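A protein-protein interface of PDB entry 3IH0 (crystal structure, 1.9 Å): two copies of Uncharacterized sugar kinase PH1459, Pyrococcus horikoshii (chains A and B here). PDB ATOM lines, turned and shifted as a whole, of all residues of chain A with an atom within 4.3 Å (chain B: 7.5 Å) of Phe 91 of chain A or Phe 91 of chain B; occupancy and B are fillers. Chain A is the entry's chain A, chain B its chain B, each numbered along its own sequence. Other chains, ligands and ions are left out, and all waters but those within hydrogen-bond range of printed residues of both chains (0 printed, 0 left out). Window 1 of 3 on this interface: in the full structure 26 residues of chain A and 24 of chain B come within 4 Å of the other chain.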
ATOM      1  N   LEU A  14      23.809 -25.046 -23.503  1.00  0.00           N
ATOM      2  CA  LEU A  14      24.116 -23.626 -23.435  1.00  0.00           C
ATOM      3  C   LEU A  14      23.932 -23.301 -21.959  1.00  0.00           C
ATOM      4  O   LEU A  14      22.811 -23.126 -21.472  1.00  0.00           O
ATOM      5  CB  LEU A  14      23.171 -22.844 -24.344  1.00  0.00           C
ATOM      6  CG  LEU A  14      23.522 -23.185 -25.802  1.00  0.00           C
ATOM      7  CD1 LEU A  14      22.323 -22.994 -26.684  1.00  0.00           C
ATOM      8  CD2 LEU A  14      24.703 -22.359 -26.264  1.00  0.00           C
ATOM      9  N   LEU A  22      16.091 -18.429 -16.313  1.00  0.00           N
ATOM     10  CA  LEU A  22      16.524 -18.487 -17.703  1.00  0.00           C
ATOM     11  C   LEU A  22      16.006 -17.271 -18.459  1.00  0.00           C
ATOM     12  O   LEU A  22      16.663 -16.784 -19.365  1.00  0.00           O
ATOM     13  CB  LEU A  22      16.028 -19.764 -18.377  1.00  0.00           C
ATOM     14  CG  LEU A  22      16.840 -21.009 -18.009  1.00  0.00           C
ATOM     15  CD1 LEU A  22      16.170 -22.252 -18.583  1.00  0.00           C
ATOM     16  CD2 LEU A  22      18.272 -20.862 -18.535  1.00  0.00           C
ATOM     17  N   PHE A  28      25.497 -17.175 -22.130  1.00  0.00           N
ATOM     18  CA  PHE A  28      25.497 -18.641 -22.148  1.00  0.00           C
ATOM     19  C   PHE A  28      26.789 -19.186 -22.765  1.00  0.00           C
ATOM     20  O   PHE A  28      27.257 -18.658 -23.774  1.00  0.00           O
ATOM     21  CB  PHE A  28      24.319 -19.156 -22.985  1.00  0.00           C
ATOM     22  CG  PHE A  28      22.973 -18.821 -22.423  1.00  0.00           C
ATOM     23  CD1 PHE A  28      22.357 -19.664 -21.501  1.00  0.00           C
ATOM     24  CD2 PHE A  28      22.332 -17.645 -22.792  1.00  0.00           C
ATOM     25  CE1 PHE A  28      21.129 -19.335 -20.953  1.00  0.00           C
ATOM     26  CE2 PHE A  28      21.104 -17.301 -22.251  1.00  0.00           C
ATOM     27  CZ  PHE A  28      20.497 -18.147 -21.328  1.00  0.00           C
ATOM     28  N   PHE A  61      26.782 -26.705 -35.346  1.00  0.00           N
ATOM     29  CA  PHE A  61      26.769 -27.365 -34.040  1.00  0.00           C
ATOM     30  C   PHE A  61      26.866 -28.880 -34.154  1.00  0.00           C
ATOM     31  O   PHE A  61      27.412 -29.534 -33.266  1.00  0.00           O
ATOM     32  CB  PHE A  61      25.528 -26.964 -33.241  1.00  0.00           C
ATOM     33  CG  PHE A  61      25.561 -25.531 -32.763  1.00  0.00           C
ATOM     34  CD1 PHE A  61      26.749 -24.805 -32.786  1.00  0.00           C
ATOM     35  CD2 PHE A  61      24.410 -24.920 -32.274  1.00  0.00           C
ATOM     36  CE1 PHE A  61      26.795 -23.491 -32.335  1.00  0.00           C
ATOM     37  CE2 PHE A  61      24.441 -23.603 -31.817  1.00  0.00           C
ATOM     38  CZ  PHE A  61      25.634 -22.888 -31.847  1.00  0.00           C
ATOM     39  N   ILE A  89      19.537 -28.650 -28.815  1.00  0.00           N
ATOM     40  CA  ILE A  89      20.081 -27.622 -27.940  1.00  0.00           C
ATOM     41  C   ILE A  89      19.239 -27.517 -26.677  1.00  0.00           C
ATOM     42  O   ILE A  89      18.028 -27.759 -26.691  1.00  0.00           O
ATOM     43  CB  ILE A  89      20.085 -26.228 -28.614  1.00  0.00           C
ATOM     44  CG1 ILE A  89      18.657 -25.857 -28.990  1.00  0.00           C
ATOM     45  CG2 ILE A  89      20.993 -26.223 -29.841  1.00  0.00           C
ATOM     46  CD1 ILE A  89      18.556 -24.569 -29.740  1.00  0.00           C
ATOM     47  N   VAL A  90      19.894 -27.162 -25.581  1.00  0.00           N
ATOM     48  CA  VAL A  90      19.210 -26.994 -24.319  1.00  0.00           C
ATOM     49  C   VAL A  90      19.882 -25.850 -23.575  1.00  0.00           C
ATOM     50  O   VAL A  90      21.117 -25.783 -23.474  1.00  0.00           O
ATOM     51  CB  VAL A  90      19.243 -28.295 -23.459  1.00  0.00           C
ATOM     52  CG1 VAL A  90      20.660 -28.785 -23.305  1.00  0.00           C
ATOM     53  CG2 VAL A  90      18.618 -28.031 -22.075  1.00  0.00           C
ATOM     54  N   PHE A  91      19.061 -24.921 -23.108  1.00  0.00           N
ATOM     55  CA  PHE A  91      19.547 -23.777 -22.366  1.00  0.00           C
ATOM     56  C   PHE A  91      19.452 -24.224 -20.923  1.00  0.00           C
ATOM     57  O   PHE A  91      18.390 -24.661 -20.473  1.00  0.00           O
ATOM     58  CB  PHE A  91      18.670 -22.568 -22.670  1.00  0.00           C
ATOM     59  CG  PHE A  91      18.874 -22.033 -24.058  1.00  0.00           C
ATOM     60  CD1 PHE A  91      19.894 -21.119 -24.326  1.00  0.00           C
ATOM     61  CD2 PHE A  91      18.080 -22.477 -25.108  1.00  0.00           C
ATOM     62  CE1 PHE A  91      20.122 -20.664 -25.627  1.00  0.00           C
ATOM     63  CE2 PHE A  91      18.299 -22.033 -26.410  1.00  0.00           C
ATOM     64  CZ  PHE A  91      19.322 -21.119 -26.671  1.00  0.00           C
ATOM     65  N   VAL A  92      20.571 -24.125 -20.221  1.00  0.00           N
ATOM     66  CA  VAL A  92      20.667 -24.597 -18.851  1.00  0.00           C
ATOM     67  C   VAL A  92      21.052 -23.611 -17.746  1.00  0.00           C
ATOM     68  O   VAL A  92      21.931 -22.768 -17.916  1.00  0.00           O
ATOM     69  CB  VAL A  92      21.680 -25.768 -18.781  1.00  0.00           C
ATOM     70  CG1 VAL A  92      21.692 -26.375 -17.375  1.00  0.00           C
ATOM     71  CG2 VAL A  92      21.346 -26.820 -19.844  1.00  0.00           C
ATOM     72  N   PHE A 101      15.931 -25.789 -16.931  1.00  0.00           N
ATOM     73  CA  PHE A 101      16.373 -25.888 -18.312  1.00  0.00           C
ATOM     74  C   PHE A 101      15.265 -25.654 -19.324  1.00  0.00           C
ATOM     75  O   PHE A 101      14.078 -25.728 -19.010  1.00  0.00           O
ATOM     76  CB  PHE A 101      17.035 -27.253 -18.562  1.00  0.00           C
ATOM     77  CG  PHE A 101      16.085 -28.421 -18.551  1.00  0.00           C
ATOM     78  CD1 PHE A 101      15.250 -28.679 -19.639  1.00  0.00           C
ATOM     79  CD2 PHE A 101      16.045 -29.283 -17.458  1.00  0.00           C
ATOM     80  CE1 PHE A 101      14.391 -29.784 -19.642  1.00  0.00           C
ATOM     81  CE2 PHE A 101      15.189 -30.395 -17.448  1.00  0.00           C
ATOM     82  CZ  PHE A 101      14.361 -30.644 -18.540  1.00  0.00           C
ATOM     83  N   LEU A 102      15.671 -25.345 -20.545  1.00  0.00           N
ATOM     84  CA  LEU A 102      14.734 -25.129 -21.636  1.00  0.00           C
ATOM     85  C   LEU A 102      15.281 -25.972 -22.773  1.00  0.00           C
ATOM     86  O   LEU A 102      16.228 -25.572 -23.453  1.00  0.00           O
ATOM     87  CB  LEU A 102      14.679 -23.651 -22.029  1.00  0.00           C
ATOM     88  CG  LEU A 102      13.827 -23.310 -23.259  1.00  0.00           C
ATOM     89  CD1 LEU A 102      12.428 -23.883 -23.120  1.00  0.00           C
ATOM     90  CD2 LEU A 102      13.766 -21.793 -23.432  1.00  0.00           C
ATOM     91  N   TYR A 104      14.936 -27.714 -26.361  1.00  0.00           N
ATOM     92  CA  TYR A 104      14.222 -27.560 -27.615  1.00  0.00           C
ATOM     93  C   TYR A 104      13.961 -28.973 -28.067  1.00  0.00           C
ATOM     94  O   TYR A 104      14.894 -29.743 -28.273  1.00  0.00           O
ATOM     95  CB  TYR A 104      15.067 -26.777 -28.611  1.00  0.00           C
ATOM     96  CG  TYR A 104      14.837 -25.304 -28.441  1.00  0.00           C
ATOM     97  CD1 TYR A 104      15.202 -24.663 -27.257  1.00  0.00           C
ATOM     98  CD2 TYR A 104      14.130 -24.574 -29.395  1.00  0.00           C
ATOM     99  CE1 TYR A 104      14.860 -23.348 -27.022  1.00  0.00           C
ATOM    100  CE2 TYR A 104      13.783 -23.252 -29.164  1.00  0.00           C
ATOM    101  CZ  TYR A 104      14.148 -22.647 -27.972  1.00  0.00           C
ATOM    102  OH  TYR A 104      13.786 -21.342 -27.708  1.00  0.00           O
ATOM    103  N   LEU B  11      12.172 -13.317 -32.222  1.00  0.00           N
ATOM    104  CA  LEU B  11      13.011 -14.367 -31.678  1.00  0.00           C
ATOM    105  C   LEU B  11      14.159 -13.896 -30.807  1.00  0.00           C
ATOM    106  O   LEU B  11      14.415 -12.691 -30.651  1.00  0.00           O
ATOM    107  CB  LEU B  11      13.566 -15.184 -32.857  1.00  0.00           C
ATOM    108  CG  LEU B  11      14.226 -14.329 -33.957  1.00  0.00           C
ATOM    109  CD1 LEU B  11      15.634 -13.919 -33.504  1.00  0.00           C
ATOM    110  CD2 LEU B  11      14.307 -15.094 -35.272  1.00  0.00           C
ATOM    111  N   ILE B  12      14.851 -14.878 -30.248  1.00  0.00           N
ATOM    112  CA  ILE B  12      16.007 -14.646 -29.409  1.00  0.00           C
ATOM    113  C   ILE B  12      17.238 -14.721 -30.312  1.00  0.00           C
ATOM    114  O   ILE B  12      17.413 -15.699 -31.036  1.00  0.00           O
ATOM    115  CB  ILE B  12      16.172 -15.754 -28.350  1.00  0.00           C
ATOM    116  CG1 ILE B  12      14.955 -15.807 -27.423  1.00  0.00           C
ATOM    117  CG2 ILE B  12      17.465 -15.534 -27.591  1.00  0.00           C
ATOM    118  CD1 ILE B  12      14.857 -14.643 -26.467  1.00  0.00           C
ATOM    119  N   ASP B  13      18.068 -13.684 -30.262  1.00  0.00           N
ATOM    120  CA  ASP B  13      19.324 -13.629 -31.010  1.00  0.00           C
ATOM    121  C   ASP B  13      20.396 -14.031 -30.010  1.00  0.00           C
ATOM    122  O   ASP B  13      20.540 -13.388 -28.971  1.00  0.00           O
ATOM    123  CB  ASP B  13      19.676 -12.194 -31.465  1.00  0.00           C
ATOM    124  CG  ASP B  13      19.250 -11.890 -32.893  1.00  0.00           C
ATOM    125  OD1 ASP B  13      18.962 -12.835 -33.649  1.00  0.00           O
ATOM    126  OD2 ASP B  13      19.226 -10.693 -33.265  1.00  0.00           O
ATOM    127  N   LEU B  14      21.132 -15.089 -30.305  1.00  0.00           N
ATOM    128  CA  LEU B  14      22.223 -15.493 -29.434  1.00  0.00           C
ATOM    129  C   LEU B  14      23.467 -15.048 -30.194  1.00  0.00           C
ATOM    130  O   LEU B  14      23.960 -15.755 -31.067  1.00  0.00           O
ATOM    131  CB  LEU B  14      22.175 -17.006 -29.218  1.00  0.00           C
ATOM    132  CG  LEU B  14      20.913 -17.263 -28.393  1.00  0.00           C
ATOM    133  CD1 LEU B  14      20.365 -18.650 -28.630  1.00  0.00           C
ATOM    134  CD2 LEU B  14      21.244 -17.013 -26.934  1.00  0.00           C
ATOM    135  N   ILE B  15      23.942 -13.841 -29.870  1.00  0.00           N
ATOM    136  CA  ILE B  15      25.094 -13.240 -30.536  1.00  0.00           C
ATOM    137  C   ILE B  15      26.466 -13.654 -30.012  1.00  0.00           C
ATOM    138  O   ILE B  15      26.750 -13.563 -28.819  1.00  0.00           O
ATOM    139  CB  ILE B  15      24.994 -11.702 -30.486  1.00  0.00           C
ATOM    140  CG1 ILE B  15      23.657 -11.264 -31.088  1.00  0.00           C
ATOM    141  CG2 ILE B  15      26.168 -11.064 -31.249  1.00  0.00           C
ATOM    142  CD1 ILE B  15      23.453  -9.772 -31.092  1.00  0.00           C
ATOM    143  N   SER B  16      27.319 -14.099 -30.927  1.00  0.00           N
ATOM    144  CA  SER B  16      28.658 -14.525 -30.569  1.00  0.00           C
ATOM    145  C   SER B  16      29.398 -13.363 -29.913  1.00  0.00           C
ATOM    146  O   SER B  16      29.347 -12.238 -30.404  1.00  0.00           O
ATOM    147  CB  SER B  16      29.401 -14.995 -31.822  1.00  0.00           C
ATOM    148  OG  SER B  16      28.685 -16.050 -32.450  1.00  0.00           O
ATOM    149  N   LEU B  22      30.802 -20.144 -36.088  1.00  0.00           N
ATOM    150  CA  LEU B  22      29.886 -20.533 -35.022  1.00  0.00           C
ATOM    151  C   LEU B  22      30.325 -21.829 -34.346  1.00  0.00           C
ATOM    152  O   LEU B  22      30.128 -22.008 -33.151  1.00  0.00           O
ATOM    153  CB  LEU B  22      28.463 -20.686 -35.559  1.00  0.00           C
ATOM    154  CG  LEU B  22      27.750 -19.362 -35.826  1.00  0.00           C
ATOM    155  CD1 LEU B  22      26.456 -19.615 -36.559  1.00  0.00           C
ATOM    156  CD2 LEU B  22      27.501 -18.652 -34.508  1.00  0.00           C
ATOM    157  N   PHE B  28      27.955 -16.720 -25.892  1.00  0.00           N
ATOM    158  CA  PHE B  28      26.872 -16.041 -26.614  1.00  0.00           C
ATOM    159  C   PHE B  28      26.093 -15.081 -25.705  1.00  0.00           C
ATOM    160  O   PHE B  28      25.910 -15.356 -24.518  1.00  0.00           O
ATOM    161  CB  PHE B  28      25.883 -17.066 -27.172  1.00  0.00           C
ATOM    162  CG  PHE B  28      26.443 -17.948 -28.243  1.00  0.00           C
ATOM    163  CD1 PHE B  28      26.365 -17.577 -29.576  1.00  0.00           C
ATOM    164  CD2 PHE B  28      27.068 -19.147 -27.917  1.00  0.00           C
ATOM    165  CE1 PHE B  28      26.870 -18.398 -30.573  1.00  0.00           C
ATOM    166  CE2 PHE B  28      27.580 -19.980 -28.906  1.00  0.00           C
ATOM    167  CZ  PHE B  28      27.493 -19.602 -30.235  1.00  0.00           C
ATOM    168  N   LYS B  30      22.446 -13.087 -25.181  1.00  0.00           N
ATOM    169  CA  LYS B  30      21.050 -13.174 -25.551  1.00  0.00           C
ATOM    170  C   LYS B  30      20.423 -11.790 -25.698  1.00  0.00           C
ATOM    171  O   LYS B  30      20.535 -10.962 -24.800  1.00  0.00           O
ATOM    172  CB  LYS B  30      20.312 -13.994 -24.490  1.00  0.00           C
ATOM    173  CG  LYS B  30      18.840 -13.718 -24.335  1.00  0.00           C
ATOM    174  CD  LYS B  30      18.184 -14.753 -23.426  1.00  0.00           C
ATOM    175  CE  LYS B  30      17.073 -14.144 -22.574  1.00  0.00           C
ATOM    176  NZ  LYS B  30      17.601 -13.365 -21.404  1.00  0.00           N
ATOM    177  N   PHE B  61      11.944 -17.745 -22.691  1.00  0.00           N
ATOM    178  CA  PHE B  61      12.362 -16.815 -23.729  1.00  0.00           C
ATOM    179  C   PHE B  61      11.191 -16.064 -24.356  1.00  0.00           C
ATOM    180  O   PHE B  61      11.329 -14.905 -24.743  1.00  0.00           O
ATOM    181  CB  PHE B  61      13.177 -17.537 -24.798  1.00  0.00           C
ATOM    182  CG  PHE B  61      14.528 -18.020 -24.315  1.00  0.00           C
ATOM    183  CD1 PHE B  61      15.050 -17.596 -23.089  1.00  0.00           C
ATOM    184  CD2 PHE B  61      15.283 -18.878 -25.100  1.00  0.00           C
ATOM    185  CE1 PHE B  61      16.295 -18.020 -22.657  1.00  0.00           C
ATOM    186  CE2 PHE B  61      16.531 -19.313 -24.680  1.00  0.00           C
ATOM    187  CZ  PHE B  61      17.045 -18.885 -23.456  1.00  0.00           C
ATOM    188  N   THR B  87      10.015 -20.749 -28.481  1.00  0.00           N
ATOM    189  CA  THR B  87      10.414 -19.446 -28.974  1.00  0.00           C
ATOM    190  C   THR B  87      11.514 -19.551 -30.013  1.00  0.00           C
ATOM    191  O   THR B  87      12.451 -20.327 -29.863  1.00  0.00           O
ATOM    192  CB  THR B  87      10.880 -18.577 -27.804  1.00  0.00           C
ATOM    193  OG1 THR B  87       9.828 -18.510 -26.833  1.00  0.00           O
ATOM    194  CG2 THR B  87      11.246 -17.170 -28.283  1.00  0.00           C
ATOM    195  N   ILE B  89      14.814 -18.984 -32.165  1.00  0.00           N
ATOM    196  CA  ILE B  89      16.166 -18.610 -31.771  1.00  0.00           C
ATOM    197  C   ILE B  89      17.067 -18.661 -32.989  1.00  0.00           C
ATOM    198  O   ILE B  89      16.815 -19.400 -33.936  1.00  0.00           O
ATOM    199  CB  ILE B  89      16.776 -19.580 -30.765  1.00  0.00           C
ATOM    200  CG1 ILE B  89      16.785 -20.969 -31.389  1.00  0.00           C
ATOM    201  CG2 ILE B  89      16.014 -19.561 -29.439  1.00  0.00           C
ATOM    202  CD1 ILE B  89      17.541 -21.953 -30.582  1.00  0.00           C
ATOM    203  N   VAL B  90      18.124 -17.874 -32.952  1.00  0.00           N
ATOM    204  CA  VAL B  90      19.093 -17.854 -34.029  1.00  0.00           C
ATOM    205  C   VAL B  90      20.451 -17.559 -33.402  1.00  0.00           C
ATOM    206  O   VAL B  90      20.578 -16.667 -32.559  1.00  0.00           O
ATOM    207  CB  VAL B  90      18.730 -16.791 -35.089  1.00  0.00           C
ATOM    208  CG1 VAL B  90      18.544 -15.459 -34.445  1.00  0.00           C
ATOM    209  CG2 VAL B  90      19.811 -16.720 -36.148  1.00  0.00           C
ATOM    210  N   PHE B  91      21.452 -18.340 -33.790  1.00  0.00           N
ATOM    211  CA  PHE B  91      22.794 -18.158 -33.277  1.00  0.00           C
ATOM    212  C   PHE B  91      23.488 -17.339 -34.326  1.00  0.00           C
ATOM    213  O   PHE B  91      23.507 -17.731 -35.492  1.00  0.00           O
ATOM    214  CB  PHE B  91      23.465 -19.517 -33.092  1.00  0.00           C
ATOM    215  CG  PHE B  91      22.883 -20.311 -31.967  1.00  0.00           C
ATOM    216  CD1 PHE B  91      23.409 -20.207 -30.679  1.00  0.00           C
ATOM    217  CD2 PHE B  91      21.767 -21.113 -32.177  1.00  0.00           C
ATOM    218  CE1 PHE B  91      22.819 -20.890 -29.609  1.00  0.00           C
ATOM    219  CE2 PHE B  91      21.165 -21.800 -31.120  1.00  0.00           C
ATOM    220  CZ  PHE B  91      21.692 -21.692 -29.834  1.00  0.00           C
ATOM    221  N   VAL B  92      24.048 -16.203 -33.930  1.00  0.00           N
ATOM    222  CA  VAL B  92      24.680 -15.346 -34.917  1.00  0.00           C
ATOM    223  C   VAL B  92      26.123 -14.934 -34.681  1.00  0.00           C
ATOM    224  O   VAL B  92      26.580 -14.810 -33.549  1.00  0.00           O
ATOM    225  CB  VAL B  92      23.852 -14.058 -35.111  1.00  0.00           C
ATOM    226  CG1 VAL B  92      22.414 -14.412 -35.448  1.00  0.00           C
ATOM    227  CG2 VAL B  92      23.893 -13.215 -33.849  1.00  0.00           C
ATOM    228  N   GLN B  93      26.847 -14.757 -35.780  1.00  0.00           N
ATOM    229  CA  GLN B  93      28.223 -14.283 -35.719  1.00  0.00           C
ATOM    230  C   GLN B  93      28.233 -13.069 -36.634  1.00  0.00           C
ATOM    231  O   GLN B  93      28.166 -13.198 -37.857  1.00  0.00           O
ATOM    232  CB  GLN B  93      29.215 -15.324 -36.227  1.00  0.00           C
ATOM    233  CG  GLN B  93      30.643 -14.799 -36.359  1.00  0.00           C
ATOM    234  CD  GLN B  93      31.173 -14.167 -35.078  1.00  0.00           C
ATOM    235  OE1 GLN B  93      30.832 -13.035 -34.736  1.00  0.00           O
ATOM    236  NE2 GLN B  93      32.012 -14.905 -34.363  1.00  0.00           N
ATOM    237  N   LEU B  94      28.284 -11.895 -36.023  1.00  0.00           N
ATOM    238  CA  LEU B  94      28.278 -10.638 -36.753  1.00  0.00           C
ATOM    239  C   LEU B  94      29.681 -10.183 -37.130  1.00  0.00           C
ATOM    240  O   LEU B  94      29.851  -9.404 -38.069  1.00  0.00           O
ATOM    241  CB  LEU B  94      27.608  -9.557 -35.914  1.00  0.00           C
ATOM    242  CG  LEU B  94      26.173  -9.879 -35.511  1.00  0.00           C
ATOM    243  CD1 LEU B  94      25.698  -8.854 -34.495  1.00  0.00           C
ATOM    244  CD2 LEU B  94      25.276  -9.911 -36.756  1.00  0.00           C
ATOM    245  N   SER B 100      27.811 -14.900 -40.263  1.00  0.00           N
ATOM    246  CA  SER B 100      27.012 -16.095 -40.475  1.00  0.00           C
ATOM    247  C   SER B 100      25.950 -16.275 -39.402  1.00  0.00           C
ATOM    248  O   SER B 100      25.955 -15.580 -38.384  1.00  0.00           O
ATOM    249  CB  SER B 100      27.914 -17.323 -40.492  1.00  0.00           C
ATOM    250  OG  SER B 100      28.555 -17.480 -39.241  1.00  0.00           O
ATOM    251  N   PHE B 101      25.048 -17.223 -39.631  1.00  0.00           N
ATOM    252  CA  PHE B 101      23.999 -17.483 -38.666  1.00  0.00           C
ATOM    253  C   PHE B 101      23.433 -18.892 -38.794  1.00  0.00           C
ATOM    254  O   PHE B 101      23.583 -19.549 -39.822  1.00  0.00           O
ATOM    255  CB  PHE B 101      22.882 -16.437 -38.818  1.00  0.00           C
ATOM    256  CG  PHE B 101      22.038 -16.617 -40.047  1.00  0.00           C
ATOM    257  CD1 PHE B 101      20.949 -17.481 -40.042  1.00  0.00           C
ATOM    258  CD2 PHE B 101      22.348 -15.942 -41.218  1.00  0.00           C
ATOM    259  CE1 PHE B 101      20.181 -17.673 -41.189  1.00  0.00           C
ATOM    260  CE2 PHE B 101      21.590 -16.129 -42.365  1.00  0.00           C
ATOM    261  CZ  PHE B 101      20.504 -16.999 -42.351  1.00  0.00           C
ATOM    262  N   LEU B 102      22.821 -19.351 -37.711  1.00  0.00           N
ATOM    263  CA  LEU B 102      22.184 -20.661 -37.648  1.00  0.00           C
ATOM    264  C   LEU B 102      20.816 -20.405 -37.026  1.00  0.00           C
ATOM    265  O   LEU B 102      20.710 -20.191 -35.824  1.00  0.00           O
ATOM    266  CB  LEU B 102      22.990 -21.620 -36.775  1.00  0.00           C
ATOM    267  CG  LEU B 102      22.252 -22.911 -36.427  1.00  0.00           C
ATOM    268  CD1 LEU B 102      21.819 -23.607 -37.702  1.00  0.00           C
ATOM    269  CD2 LEU B 102      23.155 -23.799 -35.585  1.00  0.00           C
ATOM    270  N   LEU B 103      19.787 -20.416 -37.866  1.00  0.00           N
ATOM    271  CA  LEU B 103      18.421 -20.152 -37.442  1.00  0.00           C
ATOM    272  C   LEU B 103      17.606 -21.427 -37.291  1.00  0.00           C
ATOM    273  O   LEU B 103      17.524 -22.239 -38.212  1.00  0.00           O
ATOM    274  CB  LEU B 103      17.751 -19.222 -38.452  1.00  0.00           C
ATOM    275  CG  LEU B 103      16.261 -18.895 -38.339  1.00  0.00           C
ATOM    276  CD1 LEU B 103      16.011 -17.567 -39.038  1.00  0.00           C
ATOM    277  CD2 LEU B 103      15.408 -19.996 -38.968  1.00  0.00           C
ATOM    278  N   TYR B 104      17.012 -21.602 -36.114  1.00  0.00           N
ATOM    279  CA  TYR B 104      16.196 -22.781 -35.845  1.00  0.00           C
ATOM    280  C   TYR B 104      14.804 -22.536 -36.407  1.00  0.00           C
ATOM    281  O   TYR B 104      14.080 -21.659 -35.949  1.00  0.00           O
ATOM    282  CB  TYR B 104      16.181 -23.071 -34.342  1.00  0.00           C
ATOM    283  CG  TYR B 104      17.401 -23.836 -33.900  1.00  0.00           C
ATOM    284  CD1 TYR B 104      18.683 -23.283 -34.024  1.00  0.00           C
ATOM    285  CD2 TYR B 104      17.290 -25.144 -33.434  1.00  0.00           C
ATOM    286  CE1 TYR B 104      19.815 -24.026 -33.708  1.00  0.00           C
ATOM    287  CE2 TYR B 104      18.405 -25.887 -33.117  1.00  0.00           C
ATOM    288  CZ  TYR B 104      19.663 -25.333 -33.262  1.00  0.00           C
ATOM    289  OH  TYR B 104      20.762 -26.133 -33.047  1.00  0.00           O
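Of the printed residues of chain B, Leu 22 of chain A touches Phe 61. Of the printed residues of chain B, Phe 61 of chain A touches Leu 22 (3.7 Å), Phe 91 (3.6 Å), Leu 102 (3.7 Å) and Tyr 104 (3.9 Å). Of the printed residues of chain B, Phe 91 of chain A touches Leu 14 (3.3 Å), Phe 61 (3.5 Å) and Phe 91 (3.99 Å). Of the printed residues of chain A, Leu 22 of chain B touches Phe 61 (3.7 Å). Leu 94 of chain B touches none of the printed residues of chain A. Leu 103 of chain B touches none of the printed residues of chain A. Of the printed residues of chain A, Tyr 104 of chain B touches Phe 61 (3.9 Å) and Ile 89 (3.2 Å). The nearest printed residue of chain A that does not touch Phe 91 of chain B is Ile 89 of chain A (4.05 Å). The nearest printed residue of chain B that does not touch Leu 22 of chain A is Lys 30 of chain B (4.1 Å).
Leu 14 of chain A touches Phe 91 of chain B, and with the chains exchanged Phe 91 of chain A touches Leu 14 of chain B. Leu 22 of chain A touches Phe 61 of chain B, and with the chains exchanged Phe 61 of chain A touches Leu 22 of chain B. Phe 61 of chain A touches Tyr 104 of chain B, and with the chains exchanged Tyr 104 of chain A touches Phe 61 of chain B. Phe 91 of chain B touches its own counterpart, Phe 91 of chain A. Of the 16 pairs that touch across the chains among the printed residues, 15 have their exchanged pair printed and touching as well.
The backbone carbonyl oxygen (O) of Val 90 of chain A lies within hydrogen-bond range of the backbone NH (N) of Leu 14 of chain A, at 2.8 Å. The backbone carbonyl oxygen of Leu 14 of chain A lies within hydrogen-bond range of the backbone NH of Val 92 of chain A (2.8 Å). The backbone NH (N) of Tyr 104 of chain A lies within hydrogen-bond range of the backbone carbonyl oxygen (O) of Ile 89 of chain A (3.1 Å). The backbone NH of Leu 14 of chain B lies within hydrogen-bond range of the backbone carbonyl oxygen of Val 90 of chain B (2.8 Å). O of Leu 14 of chain B is in hydrogen-bond range of N of Val 92 of chain B (2.9 Å). The backbone NH of Leu 102 of chain B is in hydrogen-bond range of the backbone carbonyl oxygen of Phe 91 of chain B (2.8 Å).
Of the 11 printed residues of chain A, 8 touch a printed residue of chain B. Hydrophobic or aromatic side chains of chain A that line the printed part of chain B: Leu 14, Phe 61, Ile 89, Phe 91, Leu 102 and Tyr 104. Hydrophobic or aromatic side chains of chain B that line the printed part of chain A: Leu 14, Phe 28, Phe 61, Ile 89, Phe 91, Leu 102 and Tyr 104. Among the printed residues, 16 pairs touch across the chains. Among the printed residues, no Asp or Glu carboxylate lies within 4 Å of a Lys or Arg side-chain nitrogen of the other chain.
The backbone NH (N) of Phe 28 of chain B lies within hydrogen-bond range of the backbone carbonyl oxygen (O) of Phe 28 of chain A (3.0 Å). OH of Tyr 104 of chain A is in hydrogen-bond range of O of Thr 87 of chain B.
Phe 91 of chain B touches Leu 14 of chain A. O of Leu 22 of chain A touches CE1 of Phe 61 of chain B, 3.5 Å away. CG of Phe 91 of chain B touches CE2 of Phe 61 of chain A, 3.6 Å away. Phe 61 of chain A touches Tyr 104 of chain B. Ile 89 of chain A touches Tyr 104 of chain B (CG2 to OH, 3.2 Å). CZ of Phe 91 of chain A touches CD1 of Leu 14 of chain B, 3.3 Å away. Phe 61 of chain B touches Phe 91 of chain A (CE2 to CD2, 3.5 Å). CZ of Phe 91 of chain A touches CZ of Phe 91 of chain B (3.99 Å). Leu 102 of chain A touches Phe 61 of chain B (CD2 to CD2, 3.7 Å). Ile 89 of chain B touches Tyr 104 of chain A.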
